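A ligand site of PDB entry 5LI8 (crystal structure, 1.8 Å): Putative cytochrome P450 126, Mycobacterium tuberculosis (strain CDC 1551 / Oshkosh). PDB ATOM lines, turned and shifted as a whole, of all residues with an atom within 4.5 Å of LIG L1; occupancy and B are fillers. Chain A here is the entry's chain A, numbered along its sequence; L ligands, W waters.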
ATOM      1  N   LEU A  64     -31.160  18.796 -27.911  1.00  0.00           N
ATOM      2  CA  LEU A  64     -31.040  17.394 -27.465  1.00  0.00           C
ATOM      3  C   LEU A  64     -32.067  16.483 -28.115  1.00  0.00           C
ATOM      4  O   LEU A  64     -31.777  15.309 -28.403  1.00  0.00           O
ATOM      5  CB  LEU A  64     -31.120  17.347 -25.923  1.00  0.00           C
ATOM      6  CG  LEU A  64     -29.990  18.041 -25.132  1.00  0.00           C
ATOM      7  CD1 LEU A  64     -30.310  17.952 -23.585  1.00  0.00           C
ATOM      8  CD2 LEU A  64     -28.737  17.321 -25.469  1.00  0.00           C
ATOM      9  N   LEU A  95     -20.060   5.460 -27.696  1.00  0.00           N
ATOM     10  CA  LEU A  95     -21.489   5.510 -27.844  1.00  0.00           C
ATOM     11  C   LEU A  95     -22.062   6.919 -27.882  1.00  0.00           C
ATOM     12  O   LEU A  95     -22.965   7.188 -28.668  1.00  0.00           O
ATOM     13  CB  LEU A  95     -22.170   4.786 -26.664  1.00  0.00           C
ATOM     14  CG  LEU A  95     -23.679   4.735 -26.640  1.00  0.00           C
ATOM     15  CD1 LEU A  95     -24.190   3.924 -27.793  1.00  0.00           C
ATOM     16  CD2 LEU A  95     -24.122   4.069 -25.324  1.00  0.00           C
ATOM     17  N   ASN A  96     -21.560   7.774 -27.073  1.00  0.00           N
ATOM     18  CA  ASN A  96     -22.157   9.148 -26.999  1.00  0.00           C
ATOM     19  C   ASN A  96     -21.709   9.987 -28.188  1.00  0.00           C
ATOM     20  O   ASN A  96     -22.211  11.117 -28.356  1.00  0.00           O
ATOM     21  CB  ASN A  96     -21.757   9.894 -25.744  1.00  0.00           C
ATOM     22  CG  ASN A  96     -20.252  10.120 -25.661  1.00  0.00           C
ATOM     23  OD1 ASN A  96     -19.478   9.145 -25.517  1.00  0.00           O
ATOM     24  ND2 ASN A  96     -19.828  11.379 -25.758  1.00  0.00           N
ATOM     25  N   HIS A 103     -25.691   3.954 -33.335  1.00  0.00           N
ATOM     26  CA  HIS A 103     -25.993   4.348 -31.972  1.00  0.00           C
ATOM     27  C   HIS A 103     -27.107   3.510 -31.339  1.00  0.00           C
ATOM     28  O   HIS A 103     -26.935   3.043 -30.242  1.00  0.00           O
ATOM     29  CB  HIS A 103     -26.440   5.845 -31.850  1.00  0.00           C
ATOM     30  CG  HIS A 103     -26.922   6.199 -30.489  1.00  0.00           C
ATOM     31  ND1 HIS A 103     -28.247   6.505 -30.234  1.00  0.00           N
ATOM     32  CD2 HIS A 103     -26.278   6.283 -29.293  1.00  0.00           C
ATOM     33  CE1 HIS A 103     -28.371   6.771 -28.946  1.00  0.00           C
ATOM     34  NE2 HIS A 103     -27.201   6.635 -28.358  1.00  0.00           N
ATOM     35  N   ARG A 107     -26.444   1.273 -28.000  1.00  0.00           N
ATOM     36  CA  ARG A 107     -27.117   1.703 -26.812  1.00  0.00           C
ATOM     37  C   ARG A 107     -27.986   0.488 -26.261  1.00  0.00           C
ATOM     38  O   ARG A 107     -27.954   0.198 -25.072  1.00  0.00           O
ATOM     39  CB  ARG A 107     -27.995   2.874 -27.074  1.00  0.00           C
ATOM     40  CG  ARG A 107     -28.729   3.427 -25.848  1.00  0.00           C
ATOM     41  CD  ARG A 107     -29.594   4.599 -26.161  1.00  0.00           C
ATOM     42  NE  ARG A 107     -30.467   5.036 -25.086  1.00  0.00           N
ATOM     43  CZ  ARG A 107     -30.116   5.853 -24.089  1.00  0.00           C
ATOM     44  NH1 ARG A 107     -28.912   6.342 -23.996  1.00  0.00           N
ATOM     45  NH2 ARG A 107     -31.018   6.183 -23.162  1.00  0.00           N
ATOM     46  N   MET A 157     -18.432   1.160  -7.799  1.00  0.00           N
ATOM     47  CA  MET A 157     -19.626   0.909  -8.599  1.00  0.00           C
ATOM     48  C   MET A 157     -19.261   0.683 -10.054  1.00  0.00           C
ATOM     49  O   MET A 157     -19.705  -0.291 -10.699  1.00  0.00           O
ATOM     50  CB  MET A 157     -20.594   2.071  -8.479  1.00  0.00           C
ATOM     51  CG  MET A 157     -21.844   1.860  -9.238  1.00  0.00           C
ATOM     52  SD  MET A 157     -21.731   2.769 -10.807  1.00  0.00           S
ATOM     53  CE  MET A 157     -21.761   4.434 -10.134  1.00  0.00           C
ATOM     54  N   ILE A 158     -18.456   1.594 -10.579  1.00  0.00           N
ATOM     55  CA  ILE A 158     -18.076   1.509 -11.995  1.00  0.00           C
ATOM     56  C   ILE A 158     -17.216   0.259 -12.263  1.00  0.00           C
ATOM     57  O   ILE A 158     -17.359  -0.384 -13.280  1.00  0.00           O
ATOM     58  CB  ILE A 158     -17.447   2.839 -12.497  1.00  0.00           C
ATOM     59  CG1 ILE A 158     -18.502   3.944 -12.566  1.00  0.00           C
ATOM     60  CG2 ILE A 158     -16.827   2.644 -13.872  1.00  0.00           C
ATOM     61  CD1 ILE A 158     -19.506   3.873 -13.777  1.00  0.00           C
ATOM     62  N   LEU A 161     -19.690  -2.730 -12.411  1.00  0.00           N
ATOM     63  CA  LEU A 161     -20.292  -2.650 -13.734  1.00  0.00           C
ATOM     64  C   LEU A 161     -19.408  -3.194 -14.882  1.00  0.00           C
ATOM     65  O   LEU A 161     -19.861  -3.927 -15.804  1.00  0.00           O
ATOM     66  CB  LEU A 161     -20.649  -1.135 -13.959  1.00  0.00           C
ATOM     67  CG  LEU A 161     -21.335  -0.709 -15.221  1.00  0.00           C
ATOM     68  CD1 LEU A 161     -22.787  -1.194 -15.255  1.00  0.00           C
ATOM     69  CD2 LEU A 161     -21.293   0.810 -15.309  1.00  0.00           C
ATOM     70  N   LEU A 250     -15.570   5.469 -19.545  1.00  0.00           N
ATOM     71  CA  LEU A 250     -16.675   5.340 -18.631  1.00  0.00           C
ATOM     72  C   LEU A 250     -16.142   5.211 -17.221  1.00  0.00           C
ATOM     73  O   LEU A 250     -16.668   5.822 -16.264  1.00  0.00           O
ATOM     74  CB  LEU A 250     -17.604   4.199 -19.066  1.00  0.00           C
ATOM     75  CG  LEU A 250     -18.832   3.990 -18.197  1.00  0.00           C
ATOM     76  CD1 LEU A 250     -19.787   5.267 -18.200  1.00  0.00           C
ATOM     77  CD2 LEU A 250     -19.577   2.729 -18.635  1.00  0.00           C
ATOM     78  N   GLY A 254     -17.726   8.275 -15.619  1.00  0.00           N
ATOM     79  CA  GLY A 254     -18.896   7.832 -14.835  1.00  0.00           C
ATOM     80  C   GLY A 254     -18.567   7.914 -13.322  1.00  0.00           C
ATOM     81  O   GLY A 254     -19.433   8.245 -12.517  1.00  0.00           O
ATOM     82  N   THR A 257     -18.395  12.154 -12.649  1.00  0.00           N
ATOM     83  CA  THR A 257     -19.691  12.779 -12.546  1.00  0.00           C
ATOM     84  C   THR A 257     -20.380  12.377 -11.236  1.00  0.00           C
ATOM     85  O   THR A 257     -20.886  13.222 -10.496  1.00  0.00           O
ATOM     86  CB  THR A 257     -20.617  12.411 -13.738  1.00  0.00           C
ATOM     87  OG1 THR A 257     -20.759  10.969 -13.844  1.00  0.00           O
ATOM     88  CG2 THR A 257     -20.133  13.047 -15.088  1.00  0.00           C
ATOM     89  N   THR A 258     -20.399  11.081 -10.949  1.00  0.00           N
ATOM     90  CA  THR A 258     -21.104  10.580  -9.748  1.00  0.00           C
ATOM     91  C   THR A 258     -20.492  11.140  -8.492  1.00  0.00           C
ATOM     92  O   THR A 258     -21.206  11.605  -7.580  1.00  0.00           O
ATOM     93  CB  THR A 258     -21.183   9.047  -9.759  1.00  0.00           C
ATOM     94  OG1 THR A 258     -21.739   8.619 -11.031  1.00  0.00           O
ATOM     95  CG2 THR A 258     -22.143   8.577  -8.635  1.00  0.00           C
ATOM     96  N   SER A 261     -21.533  14.696  -8.000  1.00  0.00           N
ATOM     97  CA  SER A 261     -22.882  14.838  -7.472  1.00  0.00           C
ATOM     98  C   SER A 261     -22.938  14.622  -5.962  1.00  0.00           C
ATOM     99  O   SER A 261     -23.693  15.295  -5.277  1.00  0.00           O
ATOM    100  CB  SER A 261     -23.860  13.923  -8.147  1.00  0.00           C
ATOM    101  OG  SER A 261     -23.693  12.537  -7.891  1.00  0.00           O
ATOM    102  N   PRO A 299     -23.287  17.877 -12.867  1.00  0.00           N
ATOM    103  CA  PRO A 299     -21.923  17.495 -13.015  1.00  0.00           C
ATOM    104  C   PRO A 299     -21.360  17.459 -14.409  1.00  0.00           C
ATOM    105  O   PRO A 299     -20.154  17.585 -14.597  1.00  0.00           O
ATOM    106  CB  PRO A 299     -21.856  16.108 -12.331  1.00  0.00           C
ATOM    107  CG  PRO A 299     -22.983  16.052 -11.444  1.00  0.00           C
ATOM    108  CD  PRO A 299     -24.074  16.854 -12.164  1.00  0.00           C
ATOM    109  N   SER A 300     -22.220  17.296 -15.375  1.00  0.00           N
ATOM    110  CA  SER A 300     -21.866  17.222 -16.802  1.00  0.00           C
ATOM    111  C   SER A 300     -22.608  18.385 -17.490  1.00  0.00           C
ATOM    112  O   SER A 300     -23.644  18.229 -18.106  1.00  0.00           O
ATOM    113  CB  SER A 300     -22.291  15.845 -17.352  1.00  0.00           C
ATOM    114  OG  SER A 300     -21.858  15.651 -18.647  1.00  0.00           O
ATOM    115  N   LYS A 303     -22.546  19.940 -23.589  1.00  0.00           N
ATOM    116  CA  LYS A 303     -22.331  18.931 -24.660  1.00  0.00           C
ATOM    117  C   LYS A 303     -22.005  19.543 -26.036  1.00  0.00           C
ATOM    118  O   LYS A 303     -22.369  20.687 -26.320  1.00  0.00           O
ATOM    119  CB  LYS A 303     -23.549  18.059 -24.856  1.00  0.00           C
ATOM    120  CG  LYS A 303     -24.036  17.403 -23.561  1.00  0.00           C
ATOM    121  CD  LYS A 303     -23.098  16.281 -23.194  1.00  0.00           C
ATOM    122  CE  LYS A 303     -23.504  15.775 -21.797  1.00  0.00           C
ATOM    123  NZ  LYS A 303     -23.300  16.791 -20.791  1.00  0.00           N
ATOM    124  N   ARG A 305     -22.529  19.164 -30.204  1.00  0.00           N
ATOM    125  CA  ARG A 305     -23.257  18.609 -31.303  1.00  0.00           C
ATOM    126  C   ARG A 305     -22.724  19.277 -32.598  1.00  0.00           C
ATOM    127  O   ARG A 305     -21.934  20.258 -32.524  1.00  0.00           O
ATOM    128  CB  ARG A 305     -24.737  18.886 -31.182  1.00  0.00           C
ATOM    129  CG  ARG A 305     -25.514  18.241 -30.051  1.00  0.00           C
ATOM    130  CD  ARG A 305     -25.419  16.736 -30.078  1.00  0.00           C
ATOM    131  NE  ARG A 305     -26.297  16.107 -29.102  1.00  0.00           N
ATOM    132  CZ  ARG A 305     -25.909  15.601 -27.919  1.00  0.00           C
ATOM    133  NH1 ARG A 305     -24.676  15.652 -27.510  1.00  0.00           N
ATOM    134  NH2 ARG A 305     -26.830  15.018 -27.141  1.00  0.00           N
ATOM    135  N   GLU A 328     -26.223  22.469 -20.328  1.00  0.00           N
ATOM    136  CA  GLU A 328     -27.250  22.053 -19.360  1.00  0.00           C
ATOM    137  C   GLU A 328     -27.094  22.693 -17.990  1.00  0.00           C
ATOM    138  O   GLU A 328     -28.084  22.880 -17.256  1.00  0.00           O
ATOM    139  CB  GLU A 328     -27.305  20.500 -19.235  1.00  0.00           C
ATOM    140  CG  GLU A 328     -27.422  19.778 -20.469  1.00  0.00           C
ATOM    141  CD  GLU A 328     -26.024  19.260 -20.923  1.00  0.00           C
ATOM    142  OE1 GLU A 328     -25.132  20.067 -21.367  1.00  0.00           O
ATOM    143  OE2 GLU A 328     -25.808  17.992 -20.847  1.00  0.00           O
ATOM    144  N   LEU A 354     -32.202  18.742 -16.816  1.00  0.00           N
ATOM    145  CA  LEU A 354     -31.451  18.107 -17.875  1.00  0.00           C
ATOM    146  C   LEU A 354     -30.062  17.558 -17.400  1.00  0.00           C
ATOM    147  O   LEU A 354     -29.176  17.328 -18.208  1.00  0.00           O
ATOM    148  CB  LEU A 354     -31.278  19.162 -19.002  1.00  0.00           C
ATOM    149  CG  LEU A 354     -32.529  19.818 -19.576  1.00  0.00           C
ATOM    150  CD1 LEU A 354     -32.129  20.829 -20.758  1.00  0.00           C
ATOM    151  CD2 LEU A 354     -33.575  18.711 -20.026  1.00  0.00           C
ATOM    152  N   GLY A 355     -29.890  17.328 -16.091  1.00  0.00           N
ATOM    153  CA  GLY A 355     -28.656  16.872 -15.531  1.00  0.00           C
ATOM    154  C   GLY A 355     -28.244  15.492 -16.006  1.00  0.00           C
ATOM    155  O   GLY A 355     -27.067  15.141 -15.966  1.00  0.00           O
ATOM    156  N   PHE A 356     -29.194  14.688 -16.468  1.00  0.00           N
ATOM    157  CA  PHE A 356     -28.900  13.373 -17.063  1.00  0.00           C
ATOM    158  C   PHE A 356     -29.182  13.335 -18.564  1.00  0.00           C
ATOM    159  O   PHE A 356     -29.289  12.269 -19.197  1.00  0.00           O
ATOM    160  CB  PHE A 356     -29.774  12.263 -16.403  1.00  0.00           C
ATOM    161  CG  PHE A 356     -29.378  11.911 -15.022  1.00  0.00           C
ATOM    162  CD1 PHE A 356     -28.066  11.580 -14.734  1.00  0.00           C
ATOM    163  CD2 PHE A 356     -30.313  11.885 -14.004  1.00  0.00           C
ATOM    164  CE1 PHE A 356     -27.698  11.235 -13.414  1.00  0.00           C
ATOM    165  CE2 PHE A 356     -29.935  11.544 -12.693  1.00  0.00           C
ATOM    166  CZ  PHE A 356     -28.677  11.235 -12.412  1.00  0.00           C
ATOM    167  N   GLY A 357     -29.285  14.519 -19.163  1.00  0.00           N
ATOM    168  CA  GLY A 357     -29.579  14.698 -20.569  1.00  0.00           C
ATOM    169  C   GLY A 357     -31.055  14.517 -20.880  1.00  0.00           C
ATOM    170  O   GLY A 357     -31.947  14.606 -20.050  1.00  0.00           O
ATOM    171  N   VAL A 360     -32.400  10.620 -27.093  1.00  0.00           N
ATOM    172  CA  VAL A 360     -31.834   9.321 -27.469  1.00  0.00           C
ATOM    173  C   VAL A 360     -30.525   8.973 -26.797  1.00  0.00           C
ATOM    174  O   VAL A 360     -30.190   7.744 -26.685  1.00  0.00           O
ATOM    175  CB  VAL A 360     -31.774   9.113 -28.984  1.00  0.00           C
ATOM    176  CG1 VAL A 360     -33.177   9.229 -29.741  1.00  0.00           C
ATOM    177  CG2 VAL A 360     -30.650  10.054 -29.639  1.00  0.00           C
ATOM    178  N   HIS A 361     -29.772   9.969 -26.339  1.00  0.00           N
ATOM    179  CA  HIS A 361     -28.559   9.762 -25.595  1.00  0.00           C
ATOM    180  C   HIS A 361     -28.672   9.879 -24.055  1.00  0.00           C
ATOM    181  O   HIS A 361     -27.663   9.974 -23.353  1.00  0.00           O
ATOM    182  CB  HIS A 361     -27.469  10.705 -26.104  1.00  0.00           C
ATOM    183  CG  HIS A 361     -26.961  10.399 -27.493  1.00  0.00           C
ATOM    184  ND1 HIS A 361     -25.968   9.456 -27.734  1.00  0.00           N
ATOM    185  CD2 HIS A 361     -27.304  10.924 -28.705  1.00  0.00           C
ATOM    186  CE1 HIS A 361     -25.745   9.424 -29.049  1.00  0.00           C
ATOM    187  NE2 HIS A 361     -26.535  10.295 -29.647  1.00  0.00           N
ATOM    188  N   TYR A 362     -29.898   9.887 -23.557  1.00  0.00           N
ATOM    189  CA  TYR A 362     -30.189  10.050 -22.135  1.00  0.00           C
ATOM    190  C   TYR A 362     -29.292   9.135 -21.269  1.00  0.00           C
ATOM    191  O   TYR A 362     -29.140   7.919 -21.645  1.00  0.00           O
ATOM    192  CB  TYR A 362     -31.664   9.758 -21.880  1.00  0.00           C
ATOM    193  CG  TYR A 362     -32.038   9.996 -20.409  1.00  0.00           C
ATOM    194  CD1 TYR A 362     -32.462  11.254 -19.942  1.00  0.00           C
ATOM    195  CD2 TYR A 362     -31.932   8.958 -19.470  1.00  0.00           C
ATOM    196  CE1 TYR A 362     -32.800  11.453 -18.618  1.00  0.00           C
ATOM    197  CE2 TYR A 362     -32.256   9.133 -18.121  1.00  0.00           C
ATOM    198  CZ  TYR A 362     -32.700  10.396 -17.694  1.00  0.00           C
ATOM    199  OH  TYR A 362     -33.020  10.588 -16.354  1.00  0.00           O
ATOM    200  N   CYS A 363     -28.699   9.659 -20.198  1.00  0.00           N
ATOM    201  CA  CYS A 363     -27.735   8.917 -19.375  1.00  0.00           C
ATOM    202  C   CYS A 363     -28.211   7.482 -19.018  1.00  0.00           C
ATOM    203  O   CYS A 363     -29.218   7.324 -18.386  1.00  0.00           O
ATOM    204  CB  CYS A 363     -27.541   9.591 -18.089  1.00  0.00           C
ATOM    205  SG  CYS A 363     -26.252   8.856 -17.057  1.00  0.00           S
ATOM    206  N   LEU A 364     -27.469   6.465 -19.447  1.00  0.00           N
ATOM    207  CA  LEU A 364     -27.784   5.074 -19.129  1.00  0.00           C
ATOM    208  C   LEU A 364     -27.470   4.761 -17.659  1.00  0.00           C
ATOM    209  O   LEU A 364     -27.928   3.762 -17.132  1.00  0.00           O
ATOM    210  CB  LEU A 364     -27.001   4.137 -20.038  1.00  0.00           C
ATOM    211  CG  LEU A 364     -27.550   4.086 -21.495  1.00  0.00           C
ATOM    212  CD1 LEU A 364     -26.618   3.223 -22.378  1.00  0.00           C
ATOM    213  CD2 LEU A 364     -28.966   3.625 -21.513  1.00  0.00           C
ATOM    214  N   GLY A 365     -26.688   5.633 -17.038  1.00  0.00           N
ATOM    215  CA  GLY A 365     -26.319   5.566 -15.617  1.00  0.00           C
ATOM    216  C   GLY A 365     -27.234   6.252 -14.583  1.00  0.00           C
ATOM    217  O   GLY A 365     -26.898   6.272 -13.385  1.00  0.00           O
ATOM    218  N   LEU A 368     -28.198   4.262 -11.568  1.00  0.00           N
ATOM    219  CA  LEU A 368     -26.985   3.977 -10.833  1.00  0.00           C
ATOM    220  C   LEU A 368     -26.499   5.205  -9.990  1.00  0.00           C
ATOM    221  O   LEU A 368     -26.146   5.077  -8.812  1.00  0.00           O
ATOM    222  CB  LEU A 368     -25.898   3.402 -11.768  1.00  0.00           C
ATOM    223  CG  LEU A 368     -26.168   1.967 -12.230  1.00  0.00           C
ATOM    224  CD1 LEU A 368     -25.181   1.581 -13.389  1.00  0.00           C
ATOM    225  CD2 LEU A 368     -25.894   0.952 -10.965  1.00  0.00           C
ATOM    226  N   ALA A 369     -26.490   6.391 -10.598  1.00  0.00           N
ATOM    227  CA  ALA A 369     -26.066   7.613  -9.930  1.00  0.00           C
ATOM    228  C   ALA A 369     -27.005   7.935  -8.757  1.00  0.00           C
ATOM    229  O   ALA A 369     -26.564   8.272  -7.664  1.00  0.00           O
ATOM    230  CB  ALA A 369     -25.944   8.808 -10.927  1.00  0.00           C
HETATM  231  C1  LIG L   1     -24.878   9.900 -21.017  1.00  0.00           C
HETATM  232  C2  LIG L   1     -24.815  12.733 -17.132  1.00  0.00           C
HETATM  233  C3  LIG L   1     -23.376   8.927 -14.385  1.00  0.00           C
HETATM  234  C4  LIG L   1     -23.392   6.172 -18.339  1.00  0.00           C
HETATM  235  C5  LIG L   1     -25.016  10.977 -20.234  1.00  0.00           C
HETATM  236  C6  LIG L   1     -25.512  12.298 -20.618  1.00  0.00           C
HETATM  237  C7  LIG L   1     -25.497  13.076 -19.514  1.00  0.00           C
HETATM  238  C8  LIG L   1     -24.998  12.304 -18.405  1.00  0.00           C
HETATM  239  C9  LIG L   1     -25.898  14.565 -19.346  1.00  0.00           C
HETATM  240  C10 LIG L   1     -25.968  12.613 -22.045  1.00  0.00           C
HETATM  241  C11 LIG L   1     -24.822  12.802 -23.041  1.00  0.00           C
HETATM  242  C12 LIG L   1     -25.205  13.546 -24.284  1.00  0.00           C
HETATM  243  O1  LIG L   1     -26.313  14.045 -24.426  1.00  0.00           O
HETATM  244  O2  LIG L   1     -24.377  13.661 -25.240  1.00  0.00           O
HETATM  245  C13 LIG L   1     -24.434  11.924 -16.034  1.00  0.00           C
HETATM  246  C14 LIG L   1     -24.339  12.368 -14.657  1.00  0.00           C
HETATM  247  C15 LIG L   1     -23.953  11.325 -13.883  1.00  0.00           C
HETATM  248  C16 LIG L   1     -23.783  10.225 -14.749  1.00  0.00           C
HETATM  249  C17 LIG L   1     -24.665  13.802 -14.272  1.00  0.00           C
HETATM  250  C18 LIG L   1     -23.716  11.258 -12.398  1.00  0.00           C
HETATM  251  C19 LIG L   1     -24.358  12.008 -11.499  1.00  0.00           C
HETATM  252  C20 LIG L   1     -23.280   7.852 -15.202  1.00  0.00           C
HETATM  253  C21 LIG L   1     -22.969   6.505 -14.821  1.00  0.00           C
HETATM  254  C22 LIG L   1     -22.972   5.734 -15.911  1.00  0.00           C
HETATM  255  C23 LIG L   1     -23.295   6.556 -17.059  1.00  0.00           C
HETATM  256  C24 LIG L   1     -22.699   6.135 -13.346  1.00  0.00           C
HETATM  257  C25 LIG L   1     -22.721   4.246 -16.001  1.00  0.00           C
HETATM  258  C26 LIG L   1     -23.656   3.455 -16.613  1.00  0.00           C
HETATM  259  C27 LIG L   1     -23.723   6.900 -19.469  1.00  0.00           C
HETATM  260  C28 LIG L   1     -23.654   6.405 -20.822  1.00  0.00           C
HETATM  261  C29 LIG L   1     -24.112   7.561 -21.638  1.00  0.00           C
HETATM  262  C30 LIG L   1     -24.408   8.627 -20.684  1.00  0.00           C
HETATM  263  C31 LIG L   1     -23.226   5.028 -21.364  1.00  0.00           C
HETATM  264  C32 LIG L   1     -24.272   7.670 -23.121  1.00  0.00           C
HETATM  265  C33 LIG L   1     -25.589   7.213 -23.620  1.00  0.00           C
HETATM  266  C34 LIG L   1     -25.745   7.384 -25.117  1.00  0.00           C
HETATM  267  O3  LIG L   1     -26.668   6.756 -25.672  1.00  0.00           O
HETATM  268  O4  LIG L   1     -24.937   8.145 -25.731  1.00  0.00           O
HETATM  269  N1  LIG L   1     -24.719  11.044 -18.877  1.00  0.00           N
HETATM  270  N2  LIG L   1     -24.086  10.574 -16.096  1.00  0.00           N
HETATM  271  N3  LIG L   1     -23.449   7.826 -16.556  1.00  0.00           N
HETATM  272  N4  LIG L   1     -24.165   8.226 -19.390  1.00  0.00           N
HETATM  273 FE1  LIG L   1     -24.111   9.449 -17.734  1.00  0.00          FE
HETATM  274  C1  LG2 L   2     -21.749  11.109 -18.576  1.00  0.00           C
HETATM  275  N1  LG2 L   2     -20.457  11.012 -18.837  1.00  0.00           N
HETATM  276  O1  LG2 L   2     -21.047  12.520 -21.511  1.00  0.00           O
HETATM  277 CL1  LG2 L   2     -19.462   6.000 -22.702  1.00  0.00          CL
HETATM  278  C2  LG2 L   2     -21.082   9.114 -17.947  1.00  0.00           C
HETATM  279  N2  LG2 L   2     -22.199   9.937 -18.013  1.00  0.00           N
HETATM  280  O2  LG2 L   2     -18.844  12.697 -21.626  1.00  0.00           O
HETATM  281 CL2  LG2 L   2     -16.954  10.539 -21.335  1.00  0.00          CL
HETATM  282  C3  LG2 L   2     -20.017   9.776 -18.456  1.00  0.00           C
HETATM  283  N3  LG2 L   2     -16.905  20.391 -24.394  1.00  0.00           N
HETATM  284  O3  LG2 L   2     -18.302  15.013 -23.047  1.00  0.00           O
HETATM  285  C4  LG2 L   2     -19.587  12.001 -19.444  1.00  0.00           C
HETATM  286  N4  LG2 L   2     -16.047  23.098 -24.725  1.00  0.00           N
HETATM  287  O4  LG2 L   2     -16.919  25.251 -24.868  1.00  0.00           O
HETATM  288  C5  LG2 L   2     -19.867  11.867 -21.001  1.00  0.00           C
HETATM  289  C6  LG2 L   2     -20.473  13.275 -22.686  1.00  0.00           C
HETATM  290  C7  LG2 L   2     -19.174  12.734 -22.945  1.00  0.00           C
HETATM  291  C8  LG2 L   2     -19.760  10.396 -21.440  1.00  0.00           C
HETATM  292  C9  LG2 L   2     -18.522   9.695 -21.613  1.00  0.00           C
HETATM  293  C10 LG2 L   2     -18.380   8.382 -21.996  1.00  0.00           C
HETATM  294  C11 LG2 L   2     -19.554   7.696 -22.221  1.00  0.00           C
HETATM  295  C12 LG2 L   2     -20.792   8.304 -22.063  1.00  0.00           C
HETATM  296  C13 LG2 L   2     -20.937   9.622 -21.693  1.00  0.00           C
HETATM  297  C14 LG2 L   2     -19.692  14.686 -22.578  1.00  0.00           C
HETATM  298  C15 LG2 L   2     -17.908  16.296 -23.411  1.00  0.00           C
HETATM  299  C16 LG2 L   2     -16.812  16.589 -24.237  1.00  0.00           C
HETATM  300  C17 LG2 L   2     -16.459  17.933 -24.579  1.00  0.00           C
HETATM  301  C18 LG2 L   2     -17.193  19.019 -24.091  1.00  0.00           C
HETATM  302  C19 LG2 L   2     -18.272  18.725 -23.279  1.00  0.00           C
HETATM  303  C20 LG2 L   2     -18.602  17.413 -22.954  1.00  0.00           C
HETATM  304  C21 LG2 L   2     -15.848  20.668 -25.342  1.00  0.00           C
HETATM  305  C22 LG2 L   2     -15.163  22.004 -25.142  1.00  0.00           C
HETATM  306  C23 LG2 L   2     -16.821  22.718 -23.571  1.00  0.00           C
HETATM  307  C24 LG2 L   2     -17.679  21.467 -23.803  1.00  0.00           C
HETATM  308  C25 LG2 L   2     -16.147  24.332 -25.280  1.00  0.00           C
HETATM  309  C26 LG2 L   2     -15.265  24.542 -26.451  1.00  0.00           C
HETATM  310  O   HOH W   1     -24.604  12.357 -27.729  1.00  0.00           O
HETATM  311  O   HOH W   2     -27.324  16.200 -22.440  1.00  0.00           O
HETATM  312  O   HOH W   3     -26.419  17.730 -17.956  1.00  0.00           O
HETATM  313  O   HOH W   4     -21.754  13.691 -25.908  1.00  0.00           O
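Leu 95 touches LIG L1 (O to O4, 3.7 Å). CA of Asn 96 touches O4 of LIG L1, at 3.2 Å. Met 157 touches LIG L1 (CE to C24, 3.8 Å). CD1 of Ile 158 touches C25 of LIG L1, at 3.9 Å. Leu 161 touches LIG L1 (CD2 to C26, 3.8 Å). Leu 250 touches LIG L1 (CD1 to C4, 3.7 Å). Gly 254 touches LIG L1 (O to C24, 3.98 Å). Thr 257 touches LIG L1 (OG1 to C15, 3.2 Å). Thr 258 touches LIG L1. OG of Ser 261 touches C19 of LIG L1, at 3.7 Å. CD of Pro 299 touches C17 of LIG L1, at 3.8 Å. CE of Lys 303 touches C11 of LIG L1 (3.5 Å). Glu 328 touches LIG L1. O of Gly 355 touches C17 of LIG L1, 3.2 Å away. Phe 356 touches LIG L1. N of Gly 357 touches C9 of LIG L1 (3.4 Å). O of Val 360 touches O3 of LIG L1, 3.8 Å away. Leu 364 touches LIG L1 (N to N4, 3.7 Å). Gly 365 touches LIG L1. Ala 369 touches LIG L1. The nearest printed residue that does not touch LIG L1 is Ser 300 (4.01 Å).
The side-chain sulfur of Cys 363 lies close to the backbone NH of Gly 365 (3.3 Å). The backbone NH (N) of Cys 363 sits at hydrogen-bond distance from the backbone carbonyl oxygen (O) of Phe 356, 2.9 Å away. The guanidinium group (NE) of Arg 107 is in hydrogen-bond range of the backbone carbonyl oxygen (O) of Val 360. NH1 of Arg 107 sits at hydrogen-bond distance from O of Tyr 362, 2.8 Å away. The backbone carbonyl oxygen (O) of Gly 254 sits at hydrogen-bond distance from the side-chain hydroxyl (OG1) of Thr 257 (3.3 Å). NZ of Lys 303 is in salt-bridge range of OE2 of Glu 328 (2.8 Å). The side-chain amino group (NZ) of Lys 303 sits at hydrogen-bond distance from the side-chain hydroxyl (OG) of Ser 300, at 2.8 Å. OG1 of Thr 258 sits at hydrogen-bond distance from O of Gly 254 (2.8 Å).
Water W4 bridges an oxygen (O2) of LIG L1 (2.7 Å) and the side-chain amide nitrogen of Asn 96 (3.0 Å). Water W1 lies within hydrogen-bond range of O of Asn 96, O2 of LIG L1, ND1 of His 361 and NH1 of Arg 305. Water W2 lies within hydrogen-bond range of the side-chain carboxylate (OE2) of Glu 328 (2.8 Å) and an oxygen (O1) of LIG L1 (3.1 Å).
An iron atom (FE1) of LIG L1 is bound by the side-chain sulfur (SG) of Cys 363, at 2.3 Å. A ring nitrogen (ND1) of His 361 sits at hydrogen-bond distance from an oxygen (O4) of LIG L1, 2.6 Å away. NE2 of His 103 is in hydrogen-bond range of O3 of LIG L1 (2.7 Å). O3 of LIG L1 is in salt-bridge range of NH1 of Arg 107, at 2.8 Å. The guanidinium group (NH2) of Arg 305 is in salt-bridge range of an oxygen (O1) of LIG L1, at 2.9 Å.
A nitrogen (N2) of LG2 L2 is bound to an iron atom (FE1) of LIG L1, at 2.0 Å.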
